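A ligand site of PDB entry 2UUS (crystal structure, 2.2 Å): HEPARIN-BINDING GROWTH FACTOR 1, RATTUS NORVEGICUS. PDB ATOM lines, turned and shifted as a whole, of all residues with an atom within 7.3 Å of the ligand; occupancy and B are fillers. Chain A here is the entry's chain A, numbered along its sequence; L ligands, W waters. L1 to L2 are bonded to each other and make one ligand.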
ATOM      1  N   ASN A  12      -7.064  -5.298  21.217  1.00  0.00           N
ATOM      2  CA  ASN A  12      -8.427  -4.819  21.421  1.00  0.00           C
ATOM      3  C   ASN A  12      -9.443  -5.914  21.097  1.00  0.00           C
ATOM      4  O   ASN A  12     -10.277  -6.272  21.940  1.00  0.00           O
ATOM      5  CB  ASN A  12      -8.706  -3.564  20.583  1.00  0.00           C
ATOM      6  CG  ASN A  12     -10.073  -2.958  20.852  1.00  0.00           C
ATOM      7  OD1 ASN A  12     -10.628  -3.067  21.951  1.00  0.00           O
ATOM      8  ND2 ASN A  12     -10.630  -2.312  19.840  1.00  0.00           N
ATOM      9  N   GLY A  13      -9.356  -6.460  19.878  1.00  0.00           N
ATOM     10  CA  GLY A  13     -10.249  -7.520  19.446  1.00  0.00           C
ATOM     11  C   GLY A  13      -9.514  -8.772  19.001  1.00  0.00           C
ATOM     12  O   GLY A  13     -10.144  -9.724  18.522  1.00  0.00           O
ATOM     13  N   LEU A 105      -7.708  -0.218  15.263  1.00  0.00           N
ATOM     14  CA  LEU A 105      -8.691  -1.246  14.867  1.00  0.00           C
ATOM     15  C   LEU A 105      -9.864  -1.383  15.868  1.00  0.00           C
ATOM     16  O   LEU A 105      -9.652  -1.374  17.089  1.00  0.00           O
ATOM     17  CB  LEU A 105      -8.004  -2.621  14.689  1.00  0.00           C
ATOM     18  CG  LEU A 105      -7.026  -2.864  13.521  1.00  0.00           C
ATOM     19  CD1 LEU A 105      -6.371  -4.245  13.584  1.00  0.00           C
ATOM     20  CD2 LEU A 105      -7.706  -2.679  12.163  1.00  0.00           C
ATOM     21  N   LYS A 106     -11.084  -1.514  15.360  1.00  0.00           N
ATOM     22  CA  LYS A 106     -12.283  -1.627  16.205  1.00  0.00           C
ATOM     23  C   LYS A 106     -12.409  -3.040  16.780  1.00  0.00           C
ATOM     24  O   LYS A 106     -11.713  -3.951  16.340  1.00  0.00           O
ATOM     25  CB  LYS A 106     -13.555  -1.311  15.405  1.00  0.00           C
ATOM     26  CG  LYS A 106     -13.679   0.101  14.781  1.00  0.00           C
ATOM     27  CD  LYS A 106     -14.744   0.107  13.673  1.00  0.00           C
ATOM     28  CE  LYS A 106     -15.318   1.491  13.394  1.00  0.00           C
ATOM     29  NZ  LYS A 106     -16.069   1.558  12.089  1.00  0.00           N
ATOM     30  N   LYS A 107     -13.310  -3.226  17.753  1.00  0.00           N
ATOM     31  CA  LYS A 107     -13.533  -4.555  18.316  1.00  0.00           C
ATOM     32  C   LYS A 107     -13.981  -5.558  17.236  1.00  0.00           C
ATOM     33  O   LYS A 107     -13.661  -6.740  17.317  1.00  0.00           O
ATOM     34  CB  LYS A 107     -14.552  -4.527  19.486  1.00  0.00           C
ATOM     35  CG  LYS A 107     -14.166  -3.616  20.676  1.00  0.00           C
ATOM     36  CD  LYS A 107     -14.972  -3.956  21.957  1.00  0.00           C
ATOM     37  CE  LYS A 107     -14.834  -2.896  23.061  1.00  0.00           C
ATOM     38  NZ  LYS A 107     -13.434  -2.728  23.580  1.00  0.00           N
ATOM     39  N   ASN A 108     -14.712  -5.073  16.231  1.00  0.00           N
ATOM     40  CA  ASN A 108     -15.189  -5.952  15.151  1.00  0.00           C
ATOM     41  C   ASN A 108     -14.188  -6.171  14.009  1.00  0.00           C
ATOM     42  O   ASN A 108     -14.519  -6.825  13.004  1.00  0.00           O
ATOM     43  CB  ASN A 108     -16.548  -5.486  14.602  1.00  0.00           C
ATOM     44  CG  ASN A 108     -16.444  -4.209  13.774  1.00  0.00           C
ATOM     45  OD1 ASN A 108     -15.387  -3.859  13.254  1.00  0.00           O
ATOM     46  ND2 ASN A 108     -17.568  -3.512  13.642  1.00  0.00           N
ATOM     47  N   GLY A 109     -12.982  -5.616  14.139  1.00  0.00           N
ATOM     48  CA  GLY A 109     -11.934  -5.850  13.162  1.00  0.00           C
ATOM     49  C   GLY A 109     -11.773  -4.880  11.994  1.00  0.00           C
ATOM     50  O   GLY A 109     -10.798  -4.963  11.248  1.00  0.00           O
ATOM     51  N   SER A 110     -12.726  -3.968  11.816  1.00  0.00           N
ATOM     52  CA  SER A 110     -12.593  -2.956  10.769  1.00  0.00           C
ATOM     53  C   SER A 110     -11.831  -1.748  11.313  1.00  0.00           C
ATOM     54  O   SER A 110     -11.694  -1.596  12.526  1.00  0.00           O
ATOM     55  CB  SER A 110     -13.950  -2.551  10.198  1.00  0.00           C
ATOM     56  OG  SER A 110     -14.822  -2.071  11.203  1.00  0.00           O
ATOM     57  N   LYS A 112     -10.608   1.881  12.615  1.00  0.00           N
ATOM     58  CA  LYS A 112     -11.147   3.101  13.242  1.00  0.00           C
ATOM     59  C   LYS A 112     -10.894   4.336  12.385  1.00  0.00           C
ATOM     60  O   LYS A 112      -9.954   4.364  11.592  1.00  0.00           O
ATOM     61  CB  LYS A 112     -10.564   3.309  14.658  1.00  0.00           C
ATOM     62  CG  LYS A 112     -11.526   2.830  15.751  1.00  0.00           C
ATOM     63  CD  LYS A 112     -11.092   3.253  17.130  1.00  0.00           C
ATOM     64  CE  LYS A 112     -11.683   4.590  17.537  1.00  0.00           C
ATOM     65  NZ  LYS A 112     -12.980   4.475  18.270  1.00  0.00           N
ATOM     66  N   PRO A 115     -10.666  10.801  13.550  1.00  0.00           N
ATOM     67  CA  PRO A 115     -11.465  11.651  14.454  1.00  0.00           C
ATOM     68  C   PRO A 115     -12.106  10.924  15.638  1.00  0.00           C
ATOM     69  O   PRO A 115     -12.529  11.610  16.568  1.00  0.00           O
ATOM     70  CB  PRO A 115     -12.586  12.195  13.529  1.00  0.00           C
ATOM     71  CG  PRO A 115     -12.039  12.071  12.146  1.00  0.00           C
ATOM     72  CD  PRO A 115     -11.163  10.851  12.164  1.00  0.00           C
ATOM     73  N   ARG A 116     -12.208   9.599  15.598  1.00  0.00           N
ATOM     74  CA  ARG A 116     -12.804   8.840  16.711  1.00  0.00           C
ATOM     75  C   ARG A 116     -11.792   8.164  17.648  1.00  0.00           C
ATOM     76  O   ARG A 116     -12.188   7.350  18.478  1.00  0.00           O
ATOM     77  CB  ARG A 116     -13.750   7.753  16.179  1.00  0.00           C
ATOM     78  CG  ARG A 116     -15.105   8.259  15.733  1.00  0.00           C
ATOM     79  CD  ARG A 116     -15.898   8.747  16.932  1.00  0.00           C
ATOM     80  NE  ARG A 116     -17.224   9.236  16.557  1.00  0.00           N
ATOM     81  CZ  ARG A 116     -18.338   8.517  16.663  1.00  0.00           C
ATOM     82  NH1 ARG A 116     -18.304   7.282  17.131  1.00  0.00           N
ATOM     83  NH2 ARG A 116     -19.501   9.056  16.294  1.00  0.00           N
ATOM     84  N   THR A 117     -10.511   8.490  17.499  1.00  0.00           N
ATOM     85  CA  THR A 117      -9.436   7.903  18.319  1.00  0.00           C
ATOM     86  C   THR A 117      -8.976   8.847  19.461  1.00  0.00           C
ATOM     87  O   THR A 117      -8.936  10.063  19.268  1.00  0.00           O
ATOM     88  CB  THR A 117      -8.209   7.504  17.460  1.00  0.00           C
ATOM     89  OG1 THR A 117      -7.585   8.679  16.900  1.00  0.00           O
ATOM     90  CG2 THR A 117      -8.589   6.555  16.325  1.00  0.00           C
ATOM     91  N   HIS A 118      -8.640   8.291  20.639  1.00  0.00           N
ATOM     92  CA  HIS A 118      -7.981   9.055  21.726  1.00  0.00           C
ATOM     93  C   HIS A 118      -6.867   8.281  22.450  1.00  0.00           C
ATOM     94  O   HIS A 118      -6.860   7.043  22.495  1.00  0.00           O
ATOM     95  CB  HIS A 118      -8.937   9.547  22.848  1.00  0.00           C
ATOM     96  CG  HIS A 118     -10.400   9.467  22.539  1.00  0.00           C
ATOM     97  ND1 HIS A 118     -11.057  10.424  21.811  1.00  0.00           N
ATOM     98  CD2 HIS A 118     -11.338   8.586  22.951  1.00  0.00           C
ATOM     99  CE1 HIS A 118     -12.337  10.115  21.734  1.00  0.00           C
ATOM    100  NE2 HIS A 118     -12.534   8.996  22.411  1.00  0.00           N
ATOM    101  N   TYR A 119      -5.954   9.025  23.057  1.00  0.00           N
ATOM    102  CA  TYR A 119      -4.991   8.483  24.011  1.00  0.00           C
ATOM    103  C   TYR A 119      -5.715   7.700  25.123  1.00  0.00           C
ATOM    104  O   TYR A 119      -6.703   8.178  25.679  1.00  0.00           O
ATOM    105  CB  TYR A 119      -4.186   9.639  24.627  1.00  0.00           C
ATOM    106  CG  TYR A 119      -2.970   9.233  25.410  1.00  0.00           C
ATOM    107  CD1 TYR A 119      -3.063   8.914  26.766  1.00  0.00           C
ATOM    108  CD2 TYR A 119      -1.714   9.161  24.807  1.00  0.00           C
ATOM    109  CE1 TYR A 119      -1.935   8.543  27.489  1.00  0.00           C
ATOM    110  CE2 TYR A 119      -0.585   8.787  25.520  1.00  0.00           C
ATOM    111  CZ  TYR A 119      -0.706   8.479  26.860  1.00  0.00           C
ATOM    112  OH  TYR A 119       0.403   8.112  27.581  1.00  0.00           O
ATOM    113  N   GLY A 120      -5.234   6.497  25.433  1.00  0.00           N
ATOM    114  CA  GLY A 120      -5.892   5.651  26.422  1.00  0.00           C
ATOM    115  C   GLY A 120      -6.703   4.470  25.897  1.00  0.00           C
ATOM    116  O   GLY A 120      -6.968   3.525  26.640  1.00  0.00           O
ATOM    117  N   GLN A 121      -7.105   4.514  24.635  1.00  0.00           N
ATOM    118  CA  GLN A 121      -7.929   3.453  24.072  1.00  0.00           C
ATOM    119  C   GLN A 121      -7.132   2.167  23.810  1.00  0.00           C
ATOM    120  O   GLN A 121      -5.976   2.217  23.435  1.00  0.00           O
ATOM    121  CB  GLN A 121      -8.549   3.922  22.744  1.00  0.00           C
ATOM    122  CG  GLN A 121      -9.726   4.888  22.859  1.00  0.00           C
ATOM    123  CD  GLN A 121     -10.167   5.412  21.495  1.00  0.00           C
ATOM    124  OE1 GLN A 121      -9.403   5.363  20.524  1.00  0.00           O
ATOM    125  NE2 GLN A 121     -11.394   5.924  21.414  1.00  0.00           N
ATOM    126  N   LYS A 122      -7.794   1.012  23.982  1.00  0.00           N
ATOM    127  CA  LYS A 122      -7.205  -0.280  23.581  1.00  0.00           C
ATOM    128  C   LYS A 122      -6.992  -0.369  22.058  1.00  0.00           C
ATOM    129  O   LYS A 122      -6.101  -1.093  21.573  1.00  0.00           O
ATOM    130  CB  LYS A 122      -8.135  -1.442  23.989  1.00  0.00           C
ATOM    131  CG  LYS A 122      -8.063  -1.913  25.426  1.00  0.00           C
ATOM    132  CD  LYS A 122      -9.231  -2.874  25.679  1.00  0.00           C
ATOM    133  CE  LYS A 122      -9.193  -3.520  27.043  1.00  0.00           C
ATOM    134  NZ  LYS A 122     -10.393  -4.419  27.232  1.00  0.00           N
ATOM    135  N   ALA A 123      -7.815   0.352  21.309  1.00  0.00           N
ATOM    136  CA  ALA A 123      -7.792   0.282  19.850  1.00  0.00           C
ATOM    137  C   ALA A 123      -6.496   0.777  19.207  1.00  0.00           C
ATOM    138  O   ALA A 123      -6.145   0.357  18.114  1.00  0.00           O
ATOM    139  CB  ALA A 123      -8.991   1.019  19.259  1.00  0.00           C
ATOM    140  N   ILE A 124      -5.780   1.673  19.889  1.00  0.00           N
ATOM    141  CA  ILE A 124      -4.599   2.293  19.292  1.00  0.00           C
ATOM    142  C   ILE A 124      -3.280   1.597  19.648  1.00  0.00           C
ATOM    143  O   ILE A 124      -2.219   2.009  19.193  1.00  0.00           O
ATOM    144  CB  ILE A 124      -4.491   3.815  19.638  1.00  0.00           C
ATOM    145  CG1 ILE A 124      -4.108   4.032  21.110  1.00  0.00           C
ATOM    146  CG2 ILE A 124      -5.784   4.533  19.266  1.00  0.00           C
ATOM    147  CD1 ILE A 124      -3.593   5.448  21.413  1.00  0.00           C
HETATM  148  C1  LIG L   1     -16.007   2.382  24.512  1.00  0.00           C
HETATM  149  O1  LIG L   1     -16.961   1.614  25.287  1.00  0.00           O
HETATM  150  C2  LIG L   1     -16.569   0.239  25.561  1.00  0.00           C
HETATM  151  C3  LIG L   1     -17.686  -0.378  26.466  1.00  0.00           C
HETATM  152  O2  LIG L   1     -17.410  -0.345  27.852  1.00  0.00           O
HETATM  153  S1  LIG L   1     -18.299   0.574  28.918  1.00  0.00           S
HETATM  154  O3  LIG L   1     -19.896   0.154  28.833  1.00  0.00           O
HETATM  155  O4  LIG L   1     -18.111   2.165  28.522  1.00  0.00           O
HETATM  156  O5  LIG L   1     -17.747   0.323  30.456  1.00  0.00           O
HETATM  157  C4  LIG L   1     -15.191   0.093  26.262  1.00  0.00           C
HETATM  158  O6  LIG L   1     -14.559  -1.162  26.053  1.00  0.00           O
HETATM  159  S2  LIG L   1     -14.297  -2.185  27.363  1.00  0.00           S
HETATM  160  O7  LIG L   1     -13.361  -1.435  28.506  1.00  0.00           O
HETATM  161  O8  LIG L   1     -13.508  -3.559  26.876  1.00  0.00           O
HETATM  162  O9  LIG L   1     -15.764  -2.591  28.029  1.00  0.00           O
HETATM  163  C5  LIG L   1     -14.145   1.101  25.681  1.00  0.00           C
HETATM  164  O10 LIG L   1     -12.993   1.137  26.497  1.00  0.00           O
HETATM  165  S3  LIG L   1     -11.496   0.642  25.951  1.00  0.00           S
HETATM  166  O11 LIG L   1     -10.663   1.890  25.225  1.00  0.00           O
HETATM  167  O12 LIG L   1     -10.686   0.102  27.293  1.00  0.00           O
HETATM  168  O13 LIG L   1     -11.672  -0.607  24.862  1.00  0.00           O
HETATM  169  C6  LIG L   1     -14.753   2.507  25.381  1.00  0.00           C
HETATM  170  O14 LIG L   1     -13.838   3.432  24.817  1.00  0.00           O
HETATM  171  S4  LIG L   1     -13.812   5.048  25.232  1.00  0.00           S
HETATM  172  O15 LIG L   1     -13.040   5.254  26.683  1.00  0.00           O
HETATM  173  O16 LIG L   1     -15.350   5.641  25.293  1.00  0.00           O
HETATM  174  O17 LIG L   1     -12.955   5.832  24.046  1.00  0.00           O
HETATM  175  C1  LG2 L   2     -15.508   3.468  21.712  1.00  0.00           C
HETATM  176  C2  LG2 L   2     -16.235   2.152  22.151  1.00  0.00           C
HETATM  177  C3  LG2 L   2     -16.230   1.113  21.008  1.00  0.00           C
HETATM  178  C4  LG2 L   2     -17.540   0.353  21.220  1.00  0.00           C
HETATM  179  C5  LG2 L   2     -18.495   1.361  21.894  1.00  0.00           C
HETATM  180  C6  LG2 L   2     -19.263   0.713  23.065  1.00  0.00           C
HETATM  181  O1  LG2 L   2     -16.162   4.074  20.601  1.00  0.00           O
HETATM  182  O2  LG2 L   2     -14.555   6.236  20.692  1.00  0.00           O
HETATM  183  O3  LG2 L   2     -14.290  -0.509  18.653  1.00  0.00           O
HETATM  184  O4  LG2 L   2     -18.408  -2.252  18.440  1.00  0.00           O
HETATM  185  O5  LG2 L   2     -22.620   0.789  23.508  1.00  0.00           O
HETATM  186  O6  LG2 L   2     -15.717   1.609  23.369  1.00  0.00           O
HETATM  187  O7  LG2 L   2     -17.221   6.545  21.047  1.00  0.00           O
HETATM  188  O8  LG2 L   2     -13.773   1.980  19.394  1.00  0.00           O
HETATM  189  O9  LG2 L   2     -20.509  -1.433  19.924  1.00  0.00           O
HETATM  190  O10 LG2 L   2     -21.940   2.569  25.431  1.00  0.00           O
HETATM  191  O11 LG2 L   2     -15.140   0.216  21.023  1.00  0.00           O
HETATM  192  O12 LG2 L   2     -16.317   5.896  18.614  1.00  0.00           O
HETATM  193  O13 LG2 L   2     -12.468  -0.007  20.673  1.00  0.00           O
HETATM  194  O14 LG2 L   2     -18.343  -2.568  21.100  1.00  0.00           O
HETATM  195  O15 LG2 L   2     -20.987  -0.006  25.484  1.00  0.00           O
HETATM  196  O16 LG2 L   2     -18.197  -0.038  20.025  1.00  0.00           O
HETATM  197  O17 LG2 L   2     -17.648   2.473  22.359  1.00  0.00           O
HETATM  198  O18 LG2 L   2     -20.101   1.713  23.625  1.00  0.00           O
HETATM  199  S1  LG2 L   2     -16.053   5.704  20.239  1.00  0.00           S
HETATM  200  S2  LG2 L   2     -13.892   0.432  19.949  1.00  0.00           S
HETATM  201  S3  LG2 L   2     -18.859  -1.575  19.886  1.00  0.00           S
HETATM  202  S4  LG2 L   2     -21.421   1.272  24.533  1.00  0.00           S
HETATM  203  O   HOH W   1      -8.528   1.765  27.708  1.00  0.00           O
HETATM  204  O   HOH W   2     -10.460   1.083  22.267  1.00  0.00           O
HETATM  205  O   HOH W   3     -15.093   5.611  28.622  1.00  0.00           O
HETATM  206  O   HOH W   4     -11.632   0.015  30.482  1.00  0.00           O
HETATM  207  O   HOH W   5     -12.824  -6.384  26.032  1.00  0.00           O
HETATM  208  O   HOH W   6     -16.182   1.222  17.108  1.00  0.00           O
HETATM  209  O   HOH W   7     -17.816  -0.688  32.979  1.00  0.00           O
HETATM  210  O   HOH W   8     -19.164   3.995  18.805  1.00  0.00           O
HETATM  211  O   HOH W   9     -15.091   0.219  32.517  1.00  0.00           O
HETATM  212  O   HOH W  10     -10.668   4.207  27.592  1.00  0.00           O
HETATM  213  O   HOH W  11     -14.910   8.039  23.113  1.00  0.00           O
HETATM  214  O   HOH W  12     -18.176  -2.656  23.778  1.00  0.00           O
HETATM  215  O   HOH W  13     -19.096   3.754  26.340  1.00  0.00           O
HETATM  216  O   HOH W  14     -15.646   3.916  16.661  1.00  0.00           O
HETATM  217  O   HOH W  15     -16.539  -2.518  16.627  1.00  0.00           O
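NH1 of Arg 116 is in salt-bridge range of O12 of LG2 L2. The side-chain amino group of Lys 112 is in salt-bridge range of an oxygen (O8) of LG2 L2. N of Lys 107 is in hydrogen-bond range of O3 of LG2 L2 (3.0 Å). An oxygen (O13) of LIG L1 is in salt-bridge range of the side-chain amino group (NZ) of Lys 107 (3.0 Å). An oxygen (O17) of LIG L1 is in hydrogen-bond range of the side-chain amide nitrogen (NE2) of Gln 121 (3.1 Å). An oxygen (O13) of LG2 L2 sits at hydrogen-bond distance from the side-chain amide nitrogen (ND2) of Asn 12 (3.1 Å). O11 of LIG L1 sits at hydrogen-bond distance from N of Lys 122 (3.2 Å). The side-chain amino group of Lys 122 is in salt-bridge range of an oxygen (O8) of LIG L1.
The backbone carbonyl oxygen of Arg 116 sits close to the side-chain amino group of Lys 112, 3.0 Å away. O of Arg 116 is in hydrogen-bond range of NE2 of Gln 121 (3.4 Å). NZ of Lys 107 is in hydrogen-bond range of OD1 of Asn 12, at 3.3 Å. The backbone NH (N) of His 118 is in hydrogen-bond range of the side-chain amide oxygen (OE1) of Gln 121, at 3.0 Å. ND2 of Asn 12 sits at hydrogen-bond distance from O of Leu 105 (3.1 Å). The backbone carbonyl oxygen (O) of Ala 123 sits at hydrogen-bond distance from the backbone NH (N) of Leu 105, 3.3 Å away.
CA of Lys 106 touches O3 of LG2 L2 (3.4 Å). His 118 touches the ligand. CB of Ala 123 touches O13 of LG2 L2, 3.9 Å away. Hydrophobic or aromatic side chains that line the ligand: His 118 and Ala 123.
Water W15 lies within hydrogen-bond range of an oxygen (O4) of LG2 L2 (2.6 Å), the backbone NH of Asn 108 (3.2 Å) and the backbone NH of Lys 107 (3.5 Å). Water W1 lies within hydrogen-bond range of the backbone carbonyl oxygen (O) of Gly 120 (2.6 Å) and an oxygen (O12) of LIG L1 (2.8 Å). Water W2 lies within hydrogen-bond range of an oxygen (O13) of LG2 L2, the backbone NH (N) of Ala 123 and the backbone NH (N) of Lys 122. Water W14 bridges an oxygen (O12) of LG2 L2 (2.9 Å) and the side-chain amino group (NZ) of Lys 112 (3.2 Å). Water W5 bridges an oxygen (O8) of LIG L1 (3.0 Å) and the side-chain amino group of Lys 122 (3.3 Å). Water W11 lies within hydrogen-bond range of a ring nitrogen (NE2) of His 118 (2.7 Å) and an oxygen (O2) of LG2 L2 (3.0 Å).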
